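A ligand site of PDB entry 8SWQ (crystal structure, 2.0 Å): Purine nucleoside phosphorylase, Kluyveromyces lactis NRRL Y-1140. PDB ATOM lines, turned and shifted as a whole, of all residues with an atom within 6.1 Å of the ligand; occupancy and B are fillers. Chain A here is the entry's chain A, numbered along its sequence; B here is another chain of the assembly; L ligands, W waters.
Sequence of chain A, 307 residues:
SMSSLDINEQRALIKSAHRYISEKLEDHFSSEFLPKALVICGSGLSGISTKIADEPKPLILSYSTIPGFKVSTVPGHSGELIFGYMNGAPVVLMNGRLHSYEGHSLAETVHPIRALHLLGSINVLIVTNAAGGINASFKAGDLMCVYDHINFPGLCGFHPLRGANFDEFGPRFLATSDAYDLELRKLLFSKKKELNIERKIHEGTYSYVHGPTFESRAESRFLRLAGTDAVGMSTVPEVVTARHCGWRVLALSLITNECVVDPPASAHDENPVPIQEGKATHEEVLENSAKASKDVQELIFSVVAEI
The backbone NH of Val 209 lies within hydrogen-bond range of the backbone carbonyl oxygen of Gly 232 (2.9 Å). O of Val 231 sits at hydrogen-bond distance from N of Gly 132 (2.9 Å). N of Ala 131 lies within hydrogen-bond range of O of Leu 254, 2.9 Å away. The side-chain hydroxyl of Tyr 206 is in hydrogen-bond range of the backbone NH of Met 233, 3.4 Å away. The backbone NH (N) of Thr 256 is in hydrogen-bond range of the backbone carbonyl oxygen (O) of Ala 131 (3.0 Å). OD1 of Asn 257 lies within hydrogen-bond range of OG1 of Thr 256 (2.9 Å). O of Gly 133 is in hydrogen-bond range of N of Cys 259 (3.0 Å). OH of Tyr 101 lies within hydrogen-bond range of ND1 of His 99 (3.4 Å).
Ser 43 touches the ligand (OG to C3, 3.8 Å). NE2 of His 99 touches O2 of the ligand (3.8 Å). Ala 130 touches the ligand (O to C6, 3.3 Å). Ala 131 touches the ligand. Phe 214 touches the ligand. Val 231 touches the ligand (O to N4, 3.8 Å). Gly 232 touches the ligand (CA to N4, 3.6 Å). Met 233 touches the ligand. Thr 256 touches the ligand. Cys 259 touches the ligand (SG to O3, 3.8 Å). Val 285 touches the ligand (CG2 to O1, 3.3 Å). Phe 173 of chain B touches the ligand. Of the 26 residues printed, 17 come within 4 Å of the ligand. The nearest printed residue that does not touch the ligand is Val 209 (4.9 Å).
Water W1 lies within hydrogen-bond range of the side-chain carboxylate of Glu 215 (2.7 Å), an oxygen (O3) of the ligand (2.8 Å) and the side-chain sulfur of Cys 259 (3.7 Å).
A nitrogen (N2) of the ligand sits close to the backbone NH (N) of Gly 132, 3.4 Å away. A nitrogen (N3) of the ligand sits at hydrogen-bond distance from the side-chain carboxylate (OE2) of Glu 215 (2.8 Å). OD1 of Asn 257 is in hydrogen-bond range of N2 of the ligand, 2.8 Å away. An oxygen (O1) of the ligand is in hydrogen-bond range of a ring nitrogen (ND1) of His 282 (2.8 Å). O2 of the ligand lies within hydrogen-bond range of OH of Tyr 101, 2.8 Å away.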
ATOM      1  N   SER A  43     -24.072  -6.941 -10.481  1.00  0.00           N
ATOM      2  CA  SER A  43     -22.931  -7.845 -10.194  1.00  0.00           C
ATOM      3  C   SER A  43     -22.488  -8.603 -11.451  1.00  0.00           C
ATOM      4  O   SER A  43     -23.338  -9.227 -12.064  1.00  0.00           O
ATOM      5  CB  SER A  43     -23.258  -8.804  -9.051  1.00  0.00           C
ATOM      6  OG  SER A  43     -23.425  -8.104  -7.832  1.00  0.00           O
ATOM      7  N   HIS A  99     -24.756  -1.485  -1.475  1.00  0.00           N
ATOM      8  CA  HIS A  99     -25.803  -2.333  -0.891  1.00  0.00           C
ATOM      9  C   HIS A  99     -25.945  -2.038   0.587  1.00  0.00           C
ATOM     10  O   HIS A  99     -24.962  -1.769   1.271  1.00  0.00           O
ATOM     11  CB  HIS A  99     -25.476  -3.806  -1.063  1.00  0.00           C
ATOM     12  CG  HIS A  99     -25.250  -4.219  -2.479  1.00  0.00           C
ATOM     13  ND1 HIS A  99     -24.036  -4.058  -3.111  1.00  0.00           N
ATOM     14  CD2 HIS A  99     -26.060  -4.821  -3.376  1.00  0.00           C
ATOM     15  CE1 HIS A  99     -24.116  -4.530  -4.344  1.00  0.00           C
ATOM     16  NE2 HIS A  99     -25.338  -4.991  -4.525  1.00  0.00           N
ATOM     17  N   TYR A 101     -26.506  -4.188   2.862  1.00  0.00           N
ATOM     18  CA  TYR A 101     -25.771  -5.200   3.651  1.00  0.00           C
ATOM     19  C   TYR A 101     -24.315  -4.832   3.980  1.00  0.00           C
ATOM     20  O   TYR A 101     -23.708  -5.411   4.898  1.00  0.00           O
ATOM     21  CB  TYR A 101     -25.849  -6.607   3.043  1.00  0.00           C
ATOM     22  CG  TYR A 101     -25.199  -6.766   1.685  1.00  0.00           C
ATOM     23  CD1 TYR A 101     -23.806  -6.715   1.522  1.00  0.00           C
ATOM     24  CD2 TYR A 101     -25.973  -7.001   0.558  1.00  0.00           C
ATOM     25  CE1 TYR A 101     -23.228  -6.860   0.281  1.00  0.00           C
ATOM     26  CE2 TYR A 101     -25.397  -7.155  -0.680  1.00  0.00           C
ATOM     27  CZ  TYR A 101     -24.034  -7.077  -0.820  1.00  0.00           C
ATOM     28  OH  TYR A 101     -23.488  -7.238  -2.067  1.00  0.00           O
ATOM     29  N   ASN A 129     -29.338  -6.076 -12.487  1.00  0.00           N
ATOM     30  CA  ASN A 129     -28.887  -6.803 -11.321  1.00  0.00           C
ATOM     31  C   ASN A 129     -28.784  -8.295 -11.609  1.00  0.00           C
ATOM     32  O   ASN A 129     -29.252  -8.771 -12.658  1.00  0.00           O
ATOM     33  CB  ASN A 129     -29.796  -6.541 -10.101  1.00  0.00           C
ATOM     34  CG  ASN A 129     -31.252  -6.993 -10.322  1.00  0.00           C
ATOM     35  OD1 ASN A 129     -31.516  -8.085 -10.842  1.00  0.00           O
ATOM     36  ND2 ASN A 129     -32.194  -6.154  -9.906  1.00  0.00           N
ATOM     37  N   ALA A 130     -28.155  -9.022 -10.698  1.00  0.00           N
ATOM     38  CA  ALA A 130     -28.208 -10.484 -10.725  1.00  0.00           C
ATOM     39  C   ALA A 130     -29.288 -10.863  -9.721  1.00  0.00           C
ATOM     40  O   ALA A 130     -29.561 -10.111  -8.800  1.00  0.00           O
ATOM     41  CB  ALA A 130     -26.865 -11.055 -10.306  1.00  0.00           C
ATOM     42  N   ALA A 131     -29.947 -12.001  -9.925  1.00  0.00           N
ATOM     43  CA  ALA A 131     -30.996 -12.414  -8.998  1.00  0.00           C
ATOM     44  C   ALA A 131     -31.119 -13.921  -8.952  1.00  0.00           C
ATOM     45  O   ALA A 131     -30.749 -14.611  -9.907  1.00  0.00           O
ATOM     46  CB  ALA A 131     -32.347 -11.765  -9.384  1.00  0.00           C
ATOM     47  N   GLY A 132     -31.644 -14.431  -7.842  1.00  0.00           N
ATOM     48  CA  GLY A 132     -31.917 -15.846  -7.733  1.00  0.00           C
ATOM     49  C   GLY A 132     -33.321 -16.112  -8.261  1.00  0.00           C
ATOM     50  O   GLY A 132     -34.225 -15.333  -7.990  1.00  0.00           O
ATOM     51  N   GLY A 133     -33.486 -17.195  -9.001  1.00  0.00           N
ATOM     52  CA  GLY A 133     -34.782 -17.505  -9.582  1.00  0.00           C
ATOM     53  C   GLY A 133     -35.648 -18.189  -8.555  1.00  0.00           C
ATOM     54  O   GLY A 133     -35.270 -19.220  -8.006  1.00  0.00           O
ATOM     55  N   TYR A 206     -39.729  -8.818  -8.979  1.00  0.00           N
ATOM     56  CA  TYR A 206     -38.465  -8.870  -8.274  1.00  0.00           C
ATOM     57  C   TYR A 206     -38.716  -8.545  -6.818  1.00  0.00           C
ATOM     58  O   TYR A 206     -39.456  -7.610  -6.515  1.00  0.00           O
ATOM     59  CB  TYR A 206     -37.511  -7.836  -8.885  1.00  0.00           C
ATOM     60  CG  TYR A 206     -36.184  -7.674  -8.179  1.00  0.00           C
ATOM     61  CD1 TYR A 206     -36.046  -6.788  -7.118  1.00  0.00           C
ATOM     62  CD2 TYR A 206     -35.051  -8.392  -8.583  1.00  0.00           C
ATOM     63  CE1 TYR A 206     -34.841  -6.626  -6.462  1.00  0.00           C
ATOM     64  CE2 TYR A 206     -33.827  -8.231  -7.919  1.00  0.00           C
ATOM     65  CZ  TYR A 206     -33.743  -7.343  -6.858  1.00  0.00           C
ATOM     66  OH  TYR A 206     -32.544  -7.148  -6.206  1.00  0.00           O
ATOM     67  N   VAL A 209     -34.430  -8.201  -0.801  1.00  0.00           N
ATOM     68  CA  VAL A 209     -34.157  -8.613   0.585  1.00  0.00           C
ATOM     69  C   VAL A 209     -32.793  -8.068   0.984  1.00  0.00           C
ATOM     70  O   VAL A 209     -31.973  -7.768   0.132  1.00  0.00           O
ATOM     71  CB  VAL A 209     -34.182 -10.147   0.776  1.00  0.00           C
ATOM     72  CG1 VAL A 209     -35.559 -10.710   0.379  1.00  0.00           C
ATOM     73  CG2 VAL A 209     -33.088 -10.817  -0.050  1.00  0.00           C
ATOM     74  N   THR A 213     -26.810 -12.994   3.548  1.00  0.00           N
ATOM     75  CA  THR A 213     -26.961 -14.440   3.370  1.00  0.00           C
ATOM     76  C   THR A 213     -27.811 -14.692   2.139  1.00  0.00           C
ATOM     77  O   THR A 213     -28.693 -13.908   1.811  1.00  0.00           O
ATOM     78  CB  THR A 213     -27.679 -15.090   4.569  1.00  0.00           C
ATOM     79  OG1 THR A 213     -28.776 -14.242   4.966  1.00  0.00           O
ATOM     80  CG2 THR A 213     -26.711 -15.227   5.729  1.00  0.00           C
ATOM     81  N   PHE A 214     -27.542 -15.796   1.454  1.00  0.00           N
ATOM     82  CA  PHE A 214     -28.476 -16.293   0.461  1.00  0.00           C
ATOM     83  C   PHE A 214     -29.643 -16.892   1.270  1.00  0.00           C
ATOM     84  O   PHE A 214     -29.462 -17.277   2.422  1.00  0.00           O
ATOM     85  CB  PHE A 214     -27.815 -17.361  -0.409  1.00  0.00           C
ATOM     86  CG  PHE A 214     -26.772 -16.817  -1.372  1.00  0.00           C
ATOM     87  CD1 PHE A 214     -27.144 -16.026  -2.454  1.00  0.00           C
ATOM     88  CD2 PHE A 214     -25.416 -17.130  -1.203  1.00  0.00           C
ATOM     89  CE1 PHE A 214     -26.187 -15.539  -3.357  1.00  0.00           C
ATOM     90  CE2 PHE A 214     -24.452 -16.653  -2.099  1.00  0.00           C
ATOM     91  CZ  PHE A 214     -24.828 -15.858  -3.172  1.00  0.00           C
ATOM     92  N   GLU A 215     -30.815 -16.961   0.656  1.00  0.00           N
ATOM     93  CA  GLU A 215     -32.053 -17.369   1.342  1.00  0.00           C
ATOM     94  C   GLU A 215     -32.072 -18.827   1.758  1.00  0.00           C
ATOM     95  O   GLU A 215     -31.618 -19.701   1.022  1.00  0.00           O
ATOM     96  CB  GLU A 215     -33.258 -17.114   0.419  1.00  0.00           C
ATOM     97  CG  GLU A 215     -33.459 -15.638   0.058  1.00  0.00           C
ATOM     98  CD  GLU A 215     -32.387 -15.110  -0.898  1.00  0.00           C
ATOM     99  OE1 GLU A 215     -32.094 -13.894  -0.817  1.00  0.00           O
ATOM    100  OE2 GLU A 215     -31.840 -15.898  -1.728  1.00  0.00           O
ATOM    101  N   VAL A 231     -35.292 -12.947  -6.701  1.00  0.00           N
ATOM    102  CA  VAL A 231     -34.917 -12.255  -5.470  1.00  0.00           C
ATOM    103  C   VAL A 231     -33.495 -11.700  -5.599  1.00  0.00           C
ATOM    104  O   VAL A 231     -32.624 -12.345  -6.164  1.00  0.00           O
ATOM    105  CB  VAL A 231     -35.022 -13.202  -4.232  1.00  0.00           C
ATOM    106  CG1 VAL A 231     -34.116 -14.446  -4.401  1.00  0.00           C
ATOM    107  CG2 VAL A 231     -34.651 -12.441  -2.929  1.00  0.00           C
ATOM    108  N   GLY A 232     -33.284 -10.486  -5.108  1.00  0.00           N
ATOM    109  CA  GLY A 232     -31.949  -9.910  -5.084  1.00  0.00           C
ATOM    110  C   GLY A 232     -31.773  -8.995  -3.880  1.00  0.00           C
ATOM    111  O   GLY A 232     -32.691  -8.857  -3.087  1.00  0.00           O
ATOM    112  N   MET A 233     -30.598  -8.368  -3.756  1.00  0.00           N
ATOM    113  CA  MET A 233     -30.302  -7.565  -2.572  1.00  0.00           C
ATOM    114  C   MET A 233     -30.115  -6.070  -2.890  1.00  0.00           C
ATOM    115  O   MET A 233     -29.393  -5.376  -2.197  1.00  0.00           O
ATOM    116  CB  MET A 233     -29.045  -8.119  -1.880  1.00  0.00           C
ATOM    117  CG  MET A 233     -29.114  -9.608  -1.529  1.00  0.00           C
ATOM    118  SD  MET A 233     -27.391 -10.165  -0.801  1.00  0.00           S
ATOM    119  CE  MET A 233     -27.659 -12.079  -0.656  1.00  0.00           C
ATOM    120  N   LEU A 254     -30.726 -10.566 -14.331  1.00  0.00           N
ATOM    121  CA  LEU A 254     -30.146 -11.784 -14.876  1.00  0.00           C
ATOM    122  C   LEU A 254     -30.299 -12.884 -13.833  1.00  0.00           C
ATOM    123  O   LEU A 254     -29.872 -12.731 -12.681  1.00  0.00           O
ATOM    124  CB  LEU A 254     -28.663 -11.580 -15.163  1.00  0.00           C
ATOM    125  CG  LEU A 254     -27.926 -12.893 -15.463  1.00  0.00           C
ATOM    126  CD1 LEU A 254     -28.505 -13.666 -16.693  1.00  0.00           C
ATOM    127  CD2 LEU A 254     -26.469 -12.601 -15.672  1.00  0.00           C
ATOM    128  N   THR A 256     -29.067 -15.756 -12.139  1.00  0.00           N
ATOM    129  CA  THR A 256     -27.737 -16.324 -12.064  1.00  0.00           C
ATOM    130  C   THR A 256     -27.708 -17.660 -11.357  1.00  0.00           C
ATOM    131  O   THR A 256     -26.685 -18.361 -11.382  1.00  0.00           O
ATOM    132  CB  THR A 256     -26.776 -15.358 -11.361  1.00  0.00           C
ATOM    133  OG1 THR A 256     -27.344 -14.953 -10.114  1.00  0.00           O
ATOM    134  CG2 THR A 256     -26.585 -14.123 -12.238  1.00  0.00           C
ATOM    135  N   ASN A 257     -28.824 -18.035 -10.742  1.00  0.00           N
ATOM    136  CA  ASN A 257     -28.926 -19.273  -9.968  1.00  0.00           C
ATOM    137  C   ASN A 257     -30.391 -19.574  -9.666  1.00  0.00           C
ATOM    138  O   ASN A 257     -31.224 -18.664  -9.657  1.00  0.00           O
ATOM    139  CB  ASN A 257     -28.100 -19.163  -8.660  1.00  0.00           C
ATOM    140  CG  ASN A 257     -28.520 -17.980  -7.791  1.00  0.00           C
ATOM    141  OD1 ASN A 257     -28.300 -16.811  -8.150  1.00  0.00           O
ATOM    142  ND2 ASN A 257     -29.124 -18.280  -6.631  1.00  0.00           N
ATOM    143  N   CYS A 259     -32.934 -20.667  -6.883  1.00  0.00           N
ATOM    144  CA  CYS A 259     -32.996 -20.766  -5.420  1.00  0.00           C
ATOM    145  C   CYS A 259     -33.439 -22.151  -4.996  1.00  0.00           C
ATOM    146  O   CYS A 259     -34.303 -22.778  -5.625  1.00  0.00           O
ATOM    147  CB  CYS A 259     -33.951 -19.722  -4.856  1.00  0.00           C
ATOM    148  SG  CYS A 259     -33.502 -18.035  -5.282  1.00  0.00           S
ATOM    149  N   ALA A 280     -26.291 -21.957  -3.286  1.00  0.00           N
ATOM    150  CA  ALA A 280     -25.820 -20.763  -3.963  1.00  0.00           C
ATOM    151  C   ALA A 280     -24.387 -20.444  -3.541  1.00  0.00           C
ATOM    152  O   ALA A 280     -24.014 -20.670  -2.394  1.00  0.00           O
ATOM    153  CB  ALA A 280     -26.724 -19.585  -3.635  1.00  0.00           C
ATOM    154  N   THR A 281     -23.589 -19.928  -4.474  1.00  0.00           N
ATOM    155  CA  THR A 281     -22.275 -19.392  -4.137  1.00  0.00           C
ATOM    156  C   THR A 281     -22.077 -18.103  -4.919  1.00  0.00           C
ATOM    157  O   THR A 281     -22.659 -17.923  -6.000  1.00  0.00           O
ATOM    158  CB  THR A 281     -21.121 -20.340  -4.535  1.00  0.00           C
ATOM    159  OG1 THR A 281     -21.168 -20.553  -5.939  1.00  0.00           O
ATOM    160  CG2 THR A 281     -21.216 -21.679  -3.796  1.00  0.00           C
ATOM    161  N   HIS A 282     -21.248 -17.203  -4.402  1.00  0.00           N
ATOM    162  CA  HIS A 282     -20.963 -15.957  -5.118  1.00  0.00           C
ATOM    163  C   HIS A 282     -20.251 -16.277  -6.426  1.00  0.00           C
ATOM    164  O   HIS A 282     -20.457 -15.599  -7.437  1.00  0.00           O
ATOM    165  CB  HIS A 282     -20.096 -15.009  -4.281  1.00  0.00           C
ATOM    166  CG  HIS A 282     -19.958 -13.646  -4.887  1.00  0.00           C
ATOM    167  ND1 HIS A 282     -21.030 -12.956  -5.400  1.00  0.00           N
ATOM    168  CD2 HIS A 282     -18.882 -12.833  -5.047  1.00  0.00           C
ATOM    169  CE1 HIS A 282     -20.631 -11.780  -5.865  1.00  0.00           C
ATOM    170  NE2 HIS A 282     -19.325 -11.686  -5.651  1.00  0.00           N
ATOM    171  N   VAL A 285     -22.712 -16.979  -9.118  1.00  0.00           N
ATOM    172  CA  VAL A 285     -23.357 -15.752  -9.570  1.00  0.00           C
ATOM    173  C   VAL A 285     -22.479 -14.983 -10.560  1.00  0.00           C
ATOM    174  O   VAL A 285     -22.937 -14.554 -11.620  1.00  0.00           O
ATOM    175  CB  VAL A 285     -23.681 -14.827  -8.374  1.00  0.00           C
ATOM    176  CG1 VAL A 285     -24.228 -13.468  -8.845  1.00  0.00           C
ATOM    177  CG2 VAL A 285     -24.672 -15.488  -7.431  1.00  0.00           C
ATOM    178  N   LEU A 286     -21.222 -14.789 -10.187  1.00  0.00           N
ATOM    179  CA  LEU A 286     -20.299 -14.023 -11.030  1.00  0.00           C
ATOM    180  C   LEU A 286     -20.051 -14.700 -12.378  1.00  0.00           C
ATOM    181  O   LEU A 286     -20.014 -14.029 -13.394  1.00  0.00           O
ATOM    182  CB  LEU A 286     -18.948 -13.838 -10.301  1.00  0.00           C
ATOM    183  CG  LEU A 286     -18.920 -12.913  -9.080  1.00  0.00           C
ATOM    184  CD1 LEU A 286     -17.506 -12.883  -8.503  1.00  0.00           C
ATOM    185  CD2 LEU A 286     -19.416 -11.508  -9.412  1.00  0.00           C
ATOM    186  N   PHE B 173     -20.817 -13.808   1.305  1.00  0.00           N
ATOM    187  CA  PHE B 173     -22.171 -14.271   1.024  1.00  0.00           C
ATOM    188  C   PHE B 173     -22.332 -15.725   1.416  1.00  0.00           C
ATOM    189  O   PHE B 173     -21.760 -16.617   0.806  1.00  0.00           O
ATOM    190  CB  PHE B 173     -22.503 -14.101  -0.477  1.00  0.00           C
ATOM    191  CG  PHE B 173     -22.316 -12.698  -0.964  1.00  0.00           C
ATOM    192  CD1 PHE B 173     -23.188 -11.689  -0.572  1.00  0.00           C
ATOM    193  CD2 PHE B 173     -21.256 -12.378  -1.810  1.00  0.00           C
ATOM    194  CE1 PHE B 173     -23.010 -10.383  -1.032  1.00  0.00           C
ATOM    195  CE2 PHE B 173     -21.077 -11.084  -2.275  1.00  0.00           C
ATOM    196  CZ  PHE B 173     -21.949 -10.076  -1.883  1.00  0.00           C
HETATM  197  O1  LIG L   1     -23.832 -13.191  -5.186  1.00  0.00           O
HETATM  198  C1  LIG L   1     -24.236 -12.327  -4.193  1.00  0.00           C
HETATM  199  C2  LIG L   1     -24.455 -10.838  -4.811  1.00  0.00           C
HETATM  200  C3  LIG L   1     -25.321 -10.906  -6.118  1.00  0.00           C
HETATM  201  C4  LIG L   1     -25.145 -10.108  -3.967  1.00  0.00           C
HETATM  202  O2  LIG L   1     -24.798  -8.730  -4.099  1.00  0.00           O
HETATM  203  C5  LIG L   1     -26.729 -10.300  -4.343  1.00  0.00           C
HETATM  204  N1  LIG L   1     -26.738 -10.860  -5.531  1.00  0.00           N
HETATM  205  C6  LIG L   1     -27.683 -10.787  -6.234  1.00  0.00           C
HETATM  206  C7  LIG L   1     -28.184 -12.257  -6.192  1.00  0.00           C
HETATM  207  C8  LIG L   1     -27.915 -13.282  -7.087  1.00  0.00           C
HETATM  208  N2  LIG L   1     -28.502 -14.401  -6.653  1.00  0.00           N
HETATM  209  C9  LIG L   1     -29.155 -14.158  -5.496  1.00  0.00           C
HETATM  210  C10 LIG L   1     -29.925 -14.946  -4.607  1.00  0.00           C
HETATM  211  O3  LIG L   1     -30.148 -16.250  -4.865  1.00  0.00           O
HETATM  212  N3  LIG L   1     -30.417 -14.398  -3.555  1.00  0.00           N
HETATM  213  C11 LIG L   1     -30.220 -13.109  -3.266  1.00  0.00           C
HETATM  214  N4  LIG L   1     -29.512 -12.344  -4.043  1.00  0.00           N
HETATM  215  C12 LIG L   1     -28.973 -12.843  -5.143  1.00  0.00           C
HETATM  216  O   HOH W   1     -30.718 -18.137  -2.838  1.00  0.00           O
